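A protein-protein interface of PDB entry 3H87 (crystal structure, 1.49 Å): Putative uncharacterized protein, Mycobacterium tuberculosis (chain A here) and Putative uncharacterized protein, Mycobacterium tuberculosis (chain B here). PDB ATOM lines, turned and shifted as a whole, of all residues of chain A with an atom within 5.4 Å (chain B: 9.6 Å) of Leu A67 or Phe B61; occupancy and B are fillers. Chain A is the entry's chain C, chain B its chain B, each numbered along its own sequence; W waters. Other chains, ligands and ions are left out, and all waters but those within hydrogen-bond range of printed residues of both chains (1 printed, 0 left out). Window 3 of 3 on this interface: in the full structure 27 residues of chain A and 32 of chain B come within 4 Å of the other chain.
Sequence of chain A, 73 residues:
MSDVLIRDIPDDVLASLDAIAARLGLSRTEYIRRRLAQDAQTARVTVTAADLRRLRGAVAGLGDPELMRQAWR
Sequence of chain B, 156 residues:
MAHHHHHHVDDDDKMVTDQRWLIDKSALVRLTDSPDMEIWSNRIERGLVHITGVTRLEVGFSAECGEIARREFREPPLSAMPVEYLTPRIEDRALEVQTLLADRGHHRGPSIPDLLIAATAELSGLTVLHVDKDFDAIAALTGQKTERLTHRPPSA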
ATOM      1  N   GLY A  61     -29.954 -22.600  -8.650  1.00  0.00           N
ATOM      2  CA  GLY A  61     -29.252 -21.856  -9.682  1.00  0.00           C
ATOM      3  C   GLY A  61     -28.533 -22.680 -10.753  1.00  0.00           C
ATOM      4  O   GLY A  61     -28.174 -22.152 -11.824  1.00  0.00           O
ATOM      5  N   LEU A  62     -28.336 -23.960 -10.508  1.00  0.00           N
ATOM      6  CA  LEU A  62     -27.813 -24.852 -11.569  1.00  0.00           C
ATOM      7  C   LEU A  62     -28.739 -24.901 -12.774  1.00  0.00           C
ATOM      8  O   LEU A  62     -28.308 -25.239 -13.881  1.00  0.00           O
ATOM      9  CB  LEU A  62     -27.616 -26.263 -11.027  1.00  0.00           C
ATOM     10  CG  LEU A  62     -26.551 -26.506  -9.989  1.00  0.00           C
ATOM     11  CD1 LEU A  62     -26.593 -27.956  -9.518  1.00  0.00           C
ATOM     12  CD2 LEU A  62     -25.150 -26.108 -10.515  1.00  0.00           C
ATOM     13  N   ASP A  64     -30.341 -22.166 -13.940  1.00  0.00           N
ATOM     14  CA  ASP A  64     -30.362 -20.820 -14.497  1.00  0.00           C
ATOM     15  C   ASP A  64     -29.220 -20.725 -15.516  1.00  0.00           C
ATOM     16  O   ASP A  64     -28.031 -20.663 -15.130  1.00  0.00           O
ATOM     17  CB  ASP A  64     -30.161 -19.812 -13.354  1.00  0.00           C
ATOM     18  CG  ASP A  64     -30.132 -18.368 -13.811  1.00  0.00           C
ATOM     19  OD1 ASP A  64     -29.891 -18.091 -15.005  1.00  0.00           O
ATOM     20  OD2 ASP A  64     -30.330 -17.495 -12.934  1.00  0.00           O
ATOM     21  N   PRO A  65     -29.542 -20.761 -16.821  1.00  0.00           N
ATOM     22  CA  PRO A  65     -28.457 -20.786 -17.805  1.00  0.00           C
ATOM     23  C   PRO A  65     -27.528 -19.580 -17.776  1.00  0.00           C
ATOM     24  O   PRO A  65     -26.321 -19.733 -18.091  1.00  0.00           O
ATOM     25  CB  PRO A  65     -29.186 -20.884 -19.144  1.00  0.00           C
ATOM     26  CG  PRO A  65     -30.476 -21.540 -18.820  1.00  0.00           C
ATOM     27  CD  PRO A  65     -30.851 -21.081 -17.428  1.00  0.00           C
ATOM     28  N   GLU A  66     -28.061 -18.402 -17.439  1.00  0.00           N
ATOM     29  CA  GLU A  66     -27.209 -17.212 -17.346  1.00  0.00           C
ATOM     30  C   GLU A  66     -26.227 -17.302 -16.178  1.00  0.00           C
ATOM     31  O   GLU A  66     -25.051 -16.946 -16.326  1.00  0.00           O
ATOM     32  CB  GLU A  66     -28.031 -15.934 -17.222  1.00  0.00           C
ATOM     33  CG  GLU A  66     -27.226 -14.713 -17.607  1.00  0.00           C
ATOM     34  CD  GLU A  66     -26.944 -14.659 -19.106  1.00  0.00           C
ATOM     35  OE1 GLU A  66     -27.922 -14.574 -19.887  1.00  0.00           O
ATOM     36  OE2 GLU A  66     -25.755 -14.695 -19.500  1.00  0.00           O
ATOM     37  N   LEU A  67     -26.709 -17.772 -15.027  1.00  0.00           N
ATOM     38  CA  LEU A  67     -25.807 -17.943 -13.856  1.00  0.00           C
ATOM     39  C   LEU A  67     -24.710 -18.943 -14.212  1.00  0.00           C
ATOM     40  O   LEU A  67     -23.527 -18.732 -13.891  1.00  0.00           O
ATOM     41  CB  LEU A  67     -26.571 -18.383 -12.594  1.00  0.00           C
ATOM     42  CG  LEU A  67     -25.766 -18.427 -11.278  1.00  0.00           C
ATOM     43  CD1 LEU A  67     -25.405 -16.975 -10.837  1.00  0.00           C
ATOM     44  CD2 LEU A  67     -26.462 -19.217 -10.113  1.00  0.00           C
ATOM     45  N   MET A  68     -25.067 -20.037 -14.873  1.00  0.00           N
ATOM     46  CA  MET A  68     -24.067 -21.013 -15.260  1.00  0.00           C
ATOM     47  C   MET A  68     -23.091 -20.519 -16.324  1.00  0.00           C
ATOM     48  O   MET A  68     -21.908 -20.883 -16.298  1.00  0.00           O
ATOM     49  CB  MET A  68     -24.712 -22.336 -15.676  1.00  0.00           C
ATOM     50  CG  MET A  68     -25.396 -23.068 -14.531  1.00  0.00           C
ATOM     51  SD  MET A  68     -24.277 -23.589 -13.206  1.00  0.00           S
ATOM     52  CE  MET A  68     -24.625 -22.271 -12.137  1.00  0.00           C
ATOM     53  N   ARG A  69     -23.532 -19.655 -17.229  1.00  0.00           N
ATOM     54  CA  ARG A  69     -22.596 -19.045 -18.157  1.00  0.00           C
ATOM     55  C   ARG A  69     -21.592 -18.159 -17.395  1.00  0.00           C
ATOM     56  O   ARG A  69     -20.394 -18.186 -17.682  1.00  0.00           O
ATOM     57  CB  ARG A  69     -23.328 -18.256 -19.238  1.00  0.00           C
ATOM     58  CG  ARG A  69     -23.821 -19.135 -20.391  1.00  0.00           C
ATOM     59  CD  ARG A  69     -24.308 -18.340 -21.602  1.00  0.00           C
ATOM     60  NE  ARG A  69     -25.565 -17.642 -21.351  1.00  0.00           N
ATOM     61  CZ  ARG A  69     -26.770 -18.194 -21.461  1.00  0.00           C
ATOM     62  NH1 ARG A  69     -26.897 -19.458 -21.839  1.00  0.00           N
ATOM     63  NH2 ARG A  69     -27.855 -17.471 -21.210  1.00  0.00           N
ATOM     64  N   GLN A  70     -22.070 -17.406 -16.408  1.00  0.00           N
ATOM     65  CA  GLN A  70     -21.201 -16.582 -15.561  1.00  0.00           C
ATOM     66  C   GLN A  70     -20.127 -17.410 -14.825  1.00  0.00           C
ATOM     67  O   GLN A  70     -18.953 -17.030 -14.752  1.00  0.00           O
ATOM     68  CB  GLN A  70     -22.068 -15.818 -14.554  1.00  0.00           C
ATOM     69  CG  GLN A  70     -21.297 -14.898 -13.650  1.00  0.00           C
ATOM     70  CD  GLN A  70     -22.179 -14.156 -12.655  1.00  0.00           C
ATOM     71  OE1 GLN A  70     -23.402 -14.056 -12.834  1.00  0.00           O
ATOM     72  NE2 GLN A  70     -21.560 -13.612 -11.611  1.00  0.00           N
ATOM     73  N   ALA A  71     -20.515 -18.588 -14.349  1.00  0.00           N
ATOM     74  CA  ALA A  71     -19.620 -19.487 -13.617  1.00  0.00           C
ATOM     75  C   ALA A  71     -18.414 -19.873 -14.500  1.00  0.00           C
ATOM     76  O   ALA A  71     -17.390 -20.261 -13.969  1.00  0.00           O
ATOM     77  CB  ALA A  71     -20.376 -20.769 -13.146  1.00  0.00           C
ATOM     78  N   LYS B  25     -24.833 -31.561 -13.810  1.00  0.00           N
ATOM     79  CA  LYS B  25     -25.645 -30.572 -13.098  1.00  0.00           C
ATOM     80  C   LYS B  25     -27.087 -30.528 -13.557  1.00  0.00           C
ATOM     81  O   LYS B  25     -28.008 -30.270 -12.741  1.00  0.00           O
ATOM     82  CB  LYS B  25     -25.046 -29.153 -13.185  1.00  0.00           C
ATOM     83  CG  LYS B  25     -24.897 -28.571 -14.636  1.00  0.00           C
ATOM     84  CD  LYS B  25     -24.496 -27.114 -14.601  1.00  0.00           C
ATOM     85  CE  LYS B  25     -24.234 -26.524 -15.990  1.00  0.00           C
ATOM     86  NZ  LYS B  25     -22.967 -27.106 -16.599  1.00  0.00           N
ATOM     87  N   GLY B  53     -15.396 -33.482  -9.759  1.00  0.00           N
ATOM     88  CA  GLY B  53     -14.939 -32.269  -9.071  1.00  0.00           C
ATOM     89  C   GLY B  53     -15.427 -30.989  -9.720  1.00  0.00           C
ATOM     90  O   GLY B  53     -15.759 -30.011  -9.003  1.00  0.00           O
ATOM     91  N   VAL B  54     -15.489 -30.935 -11.056  1.00  0.00           N
ATOM     92  CA  VAL B  54     -16.023 -29.757 -11.738  1.00  0.00           C
ATOM     93  C   VAL B  54     -17.493 -29.515 -11.371  1.00  0.00           C
ATOM     94  O   VAL B  54     -17.899 -28.359 -11.106  1.00  0.00           O
ATOM     95  CB  VAL B  54     -15.879 -29.954 -13.281  1.00  0.00           C
ATOM     96  CG1 VAL B  54     -16.728 -28.943 -14.102  1.00  0.00           C
ATOM     97  CG2 VAL B  54     -14.351 -29.866 -13.637  1.00  0.00           C
ATOM     98  N   THR B  55     -18.326 -30.560 -11.357  1.00  0.00           N
ATOM     99  CA  THR B  55     -19.749 -30.389 -10.983  1.00  0.00           C
ATOM    100  C   THR B  55     -19.886 -29.942  -9.511  1.00  0.00           C
ATOM    101  O   THR B  55     -20.759 -29.144  -9.185  1.00  0.00           O
ATOM    102  CB  THR B  55     -20.557 -31.676 -11.264  1.00  0.00           C
ATOM    103  OG1 THR B  55     -20.364 -32.042 -12.656  1.00  0.00           O
ATOM    104  CG2 THR B  55     -22.054 -31.513 -10.972  1.00  0.00           C
ATOM    105  N   ARG B  56     -18.992 -30.372  -8.625  1.00  0.00           N
ATOM    106  CA  ARG B  56     -18.991 -29.933  -7.238  1.00  0.00           C
ATOM    107  C   ARG B  56     -18.735 -28.418  -7.201  1.00  0.00           C
ATOM    108  O   ARG B  56     -19.360 -27.682  -6.381  1.00  0.00           O
ATOM    109  CB  ARG B  56     -18.000 -30.766  -6.394  1.00  0.00           C
ATOM    110  CG  ARG B  56     -18.491 -32.192  -6.187  1.00  0.00           C
ATOM    111  CD  ARG B  56     -17.425 -33.202  -5.704  1.00  0.00           C
ATOM    112  NE  ARG B  56     -16.754 -32.776  -4.514  1.00  0.00           N
ATOM    113  CZ  ARG B  56     -17.226 -32.982  -3.280  1.00  0.00           C
ATOM    114  NH1 ARG B  56     -18.335 -33.682  -3.031  1.00  0.00           N
ATOM    115  NH2 ARG B  56     -16.599 -32.500  -2.233  1.00  0.00           N
ATOM    116  N   LEU B  57     -17.808 -27.897  -8.013  1.00  0.00           N
ATOM    117  CA  LEU B  57     -17.588 -26.448  -8.099  1.00  0.00           C
ATOM    118  C   LEU B  57     -18.824 -25.691  -8.601  1.00  0.00           C
ATOM    119  O   LEU B  57     -19.082 -24.547  -8.213  1.00  0.00           O
ATOM    120  CB  LEU B  57     -16.336 -26.131  -8.928  1.00  0.00           C
ATOM    121  CG  LEU B  57     -15.015 -26.296  -8.208  1.00  0.00           C
ATOM    122  CD1 LEU B  57     -13.844 -26.598  -9.172  1.00  0.00           C
ATOM    123  CD2 LEU B  57     -14.743 -25.046  -7.357  1.00  0.00           C
ATOM    124  N   GLU B  58     -19.563 -26.320  -9.522  1.00  0.00           N
ATOM    125  CA  GLU B  58     -20.829 -25.727  -9.997  1.00  0.00           C
ATOM    126  C   GLU B  58     -21.881 -25.674  -8.859  1.00  0.00           C
ATOM    127  O   GLU B  58     -22.589 -24.674  -8.690  1.00  0.00           O
ATOM    128  CB  GLU B  58     -21.375 -26.468 -11.231  1.00  0.00           C
ATOM    129  CG  GLU B  58     -20.438 -26.343 -12.443  1.00  0.00           C
ATOM    130  CD  GLU B  58     -20.973 -27.075 -13.657  1.00  0.00           C
ATOM    131  OE1 GLU B  58     -21.419 -28.243 -13.450  1.00  0.00           O
ATOM    132  OE2 GLU B  58     -21.000 -26.474 -14.749  1.00  0.00           O
ATOM    133  N   VAL B  59     -21.985 -26.751  -8.082  1.00  0.00           N
ATOM    134  CA  VAL B  59     -22.825 -26.755  -6.859  1.00  0.00           C
ATOM    135  C   VAL B  59     -22.432 -25.604  -5.929  1.00  0.00           C
ATOM    136  O   VAL B  59     -23.291 -24.842  -5.466  1.00  0.00           O
ATOM    137  CB  VAL B  59     -22.723 -28.089  -6.147  1.00  0.00           C
ATOM    138  CG1 VAL B  59     -23.312 -28.028  -4.715  1.00  0.00           C
ATOM    139  CG2 VAL B  59     -23.396 -29.184  -6.971  1.00  0.00           C
ATOM    140  N   GLY B  60     -21.143 -25.405  -5.675  1.00  0.00           N
ATOM    141  CA  GLY B  60     -20.701 -24.325  -4.782  1.00  0.00           C
ATOM    142  C   GLY B  60     -21.050 -22.960  -5.332  1.00  0.00           C
ATOM    143  O   GLY B  60     -21.421 -22.041  -4.602  1.00  0.00           O
ATOM    144  N   PHE B  61     -20.892 -22.785  -6.651  1.00  0.00           N
ATOM    145  CA  PHE B  61     -21.217 -21.496  -7.288  1.00  0.00           C
ATOM    146  C   PHE B  61     -22.701 -21.172  -7.108  1.00  0.00           C
ATOM    147  O   PHE B  61     -23.100 -20.010  -6.860  1.00  0.00           O
ATOM    148  CB  PHE B  61     -20.858 -21.501  -8.814  1.00  0.00           C
ATOM    149  CG  PHE B  61     -20.811 -20.130  -9.462  1.00  0.00           C
ATOM    150  CD1 PHE B  61     -19.629 -19.396  -9.492  1.00  0.00           C
ATOM    151  CD2 PHE B  61     -21.932 -19.604 -10.074  1.00  0.00           C
ATOM    152  CE1 PHE B  61     -19.553 -18.164 -10.117  1.00  0.00           C
ATOM    153  CE2 PHE B  61     -21.862 -18.328 -10.668  1.00  0.00           C
ATOM    154  CZ  PHE B  61     -20.688 -17.627 -10.677  1.00  0.00           C
ATOM    155  N   SER B  62     -23.545 -22.199  -7.271  1.00  0.00           N
ATOM    156  CA  SER B  62     -25.003 -22.020  -7.187  1.00  0.00           C
ATOM    157  C   SER B  62     -25.496 -21.739  -5.770  1.00  0.00           C
ATOM    158  O   SER B  62     -26.542 -21.101  -5.593  1.00  0.00           O
ATOM    159  CB  SER B  62     -25.722 -23.252  -7.755  1.00  0.00           C
ATOM    160  OG  SER B  62     -25.703 -24.372  -6.886  1.00  0.00           O
ATOM    161  N   ALA B  63     -24.794 -22.229  -4.761  1.00  0.00           N
ATOM    162  CA  ALA B  63     -25.213 -22.058  -3.348  1.00  0.00           C
ATOM    163  C   ALA B  63     -25.191 -20.584  -2.966  1.00  0.00           C
ATOM    164  O   ALA B  63     -24.297 -19.850  -3.398  1.00  0.00           O
ATOM    165  CB  ALA B  63     -24.300 -22.843  -2.453  1.00  0.00           C
ATOM    166  N   GLU B  64     -26.130 -20.136  -2.128  1.00  0.00           N
ATOM    167  CA  GLU B  64     -26.220 -18.705  -1.780  1.00  0.00           C
ATOM    168  C   GLU B  64     -25.135 -18.265  -0.807  1.00  0.00           C
ATOM    169  O   GLU B  64     -24.770 -17.085  -0.782  1.00  0.00           O
ATOM    170  CB  GLU B  64     -27.601 -18.416  -1.198  1.00  0.00           C
ATOM    171  CG  GLU B  64     -28.703 -18.303  -2.241  1.00  0.00           C
ATOM    172  CD  GLU B  64     -28.498 -17.110  -3.161  1.00  0.00           C
ATOM    173  OE1 GLU B  64     -28.141 -16.023  -2.665  1.00  0.00           O
ATOM    174  OE2 GLU B  64     -28.676 -17.259  -4.389  1.00  0.00           O
ATOM    175  N   CYS B  65     -24.643 -19.181   0.013  1.00  0.00           N
ATOM    176  CA  CYS B  65     -23.552 -18.867   0.916  1.00  0.00           C
ATOM    177  C   CYS B  65     -22.750 -20.108   1.264  1.00  0.00           C
ATOM    178  O   CYS B  65     -23.107 -21.226   0.876  1.00  0.00           O
ATOM    179  CB  CYS B  65     -24.060 -18.214   2.173  1.00  0.00           C
ATOM    180  SG  CYS B  65     -24.725 -19.352   3.344  1.00  0.00           S
ATOM    181  N   GLY B  66     -21.574 -19.909   1.868  1.00  0.00           N
ATOM    182  CA  GLY B  66     -20.630 -21.000   2.090  1.00  0.00           C
ATOM    183  C   GLY B  66     -21.139 -22.078   3.040  1.00  0.00           C
ATOM    184  O   GLY B  66     -20.851 -23.272   2.827  1.00  0.00           O
ATOM    185  N   ILE B  68     -24.232 -23.073   3.377  1.00  0.00           N
ATOM    186  CA  ILE B  68     -25.198 -23.885   2.662  1.00  0.00           C
ATOM    187  C   ILE B  68     -24.425 -24.922   1.814  1.00  0.00           C
ATOM    188  O   ILE B  68     -24.773 -26.129   1.749  1.00  0.00           O
ATOM    189  CB  ILE B  68     -26.167 -23.005   1.787  1.00  0.00           C
ATOM    190  CG1 ILE B  68     -27.086 -22.170   2.681  1.00  0.00           C
ATOM    191  CG2 ILE B  68     -26.957 -23.879   0.784  1.00  0.00           C
ATOM    192  CD1 ILE B  68     -27.798 -21.021   1.945  1.00  0.00           C
ATOM    193  N   ALA B  69     -23.361 -24.499   1.138  1.00  0.00           N
ATOM    194  CA  ALA B  69     -22.512 -25.433   0.418  1.00  0.00           C
ATOM    195  C   ALA B  69     -21.910 -26.503   1.298  1.00  0.00           C
ATOM    196  O   ALA B  69     -21.960 -27.700   0.950  1.00  0.00           O
ATOM    197  CB  ALA B  69     -21.398 -24.660  -0.342  1.00  0.00           C
ATOM    198  N   PHE B  73     -22.435 -30.685   0.945  1.00  0.00           N
ATOM    199  CA  PHE B  73     -21.386 -31.667   0.705  1.00  0.00           C
ATOM    200  C   PHE B  73     -21.270 -32.708   1.818  1.00  0.00           C
ATOM    201  O   PHE B  73     -20.791 -33.817   1.546  1.00  0.00           O
ATOM    202  CB  PHE B  73     -20.026 -30.958   0.506  1.00  0.00           C
ATOM    203  CG  PHE B  73     -19.948 -30.145  -0.786  1.00  0.00           C
ATOM    204  CD1 PHE B  73     -20.252 -30.708  -2.001  1.00  0.00           C
ATOM    205  CD2 PHE B  73     -19.601 -28.807  -0.765  1.00  0.00           C
ATOM    206  CE1 PHE B  73     -20.155 -29.925  -3.188  1.00  0.00           C
ATOM    207  CE2 PHE B  73     -19.532 -28.046  -1.951  1.00  0.00           C
ATOM    208  CZ  PHE B  73     -19.825 -28.621  -3.131  1.00  0.00           C
HETATM  209  O   HOH W   1     -29.090 -21.666  -6.040  1.00  0.00           O
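Leu A62 touches Glu B58. CG of Leu A62 touches OG of Ser B62, at 3.9 Å. Leu A67 touches Phe B61. Lys B25 touches Met A68 (CD to SD, 3.8 Å). CD2 of Phe B61 touches CB of Ala A71, at 3.6 Å.
Water W1 lies within hydrogen-bond range of the backbone carbonyl oxygen of Ser B62 (2.6 Å) and the backbone NH of Gly A61 (2.9 Å).
Of chain B, only Phe B61 (3.7 Å) comes within 4 Å of Leu A67. Of the printed residues of chain A, Phe B61 touches Leu A67 (3.7 Å) and Ala A71 (3.6 Å). Asp A64 touches none of the printed residues of chain B. Printed residues of chain A within 4 Å of Lys B25: Met A68. Printed residues of chain B within 4 Å of Leu A62: Glu B58 and Ser B62. Printed residues of chain A within 4 Å of Ser B62: Leu A62 (3.9 Å). The nearest residue of chain B that does not touch Leu A67 is Ser B62 (4.3 Å). The nearest printed residue of chain A that does not touch Phe B61 is Gln A70 (4.1 Å).
The side-chain amino group of Lys B25 lies within salt-bridge range of the side-chain carboxylate of Glu B58 (2.8 Å). The side-chain hydroxyl (OG) of Ser B62 is in hydrogen-bond range of the backbone carbonyl oxygen (O) of Val B59, at 2.8 Å. The side-chain carboxylate (OD1) of Asp A64 is in hydrogen-bond range of the backbone NH (N) of Leu A67, at 3.2 Å.
Printed residues of chain A that touch a printed residue of chain B: Leu A62, Leu A67, Met A68 and Ala A71. Hydrophobic or aromatic side chains of chain A within 4 Å of the printed part of chain B: Leu A62, Leu A67, Met A68 and Ala A71. Hydrophobic or aromatic side chains of chain B that line the printed part of chain A: Phe B61. Along chain B the printed residues that touch a printed residue of chain A span positions 25 to 62.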
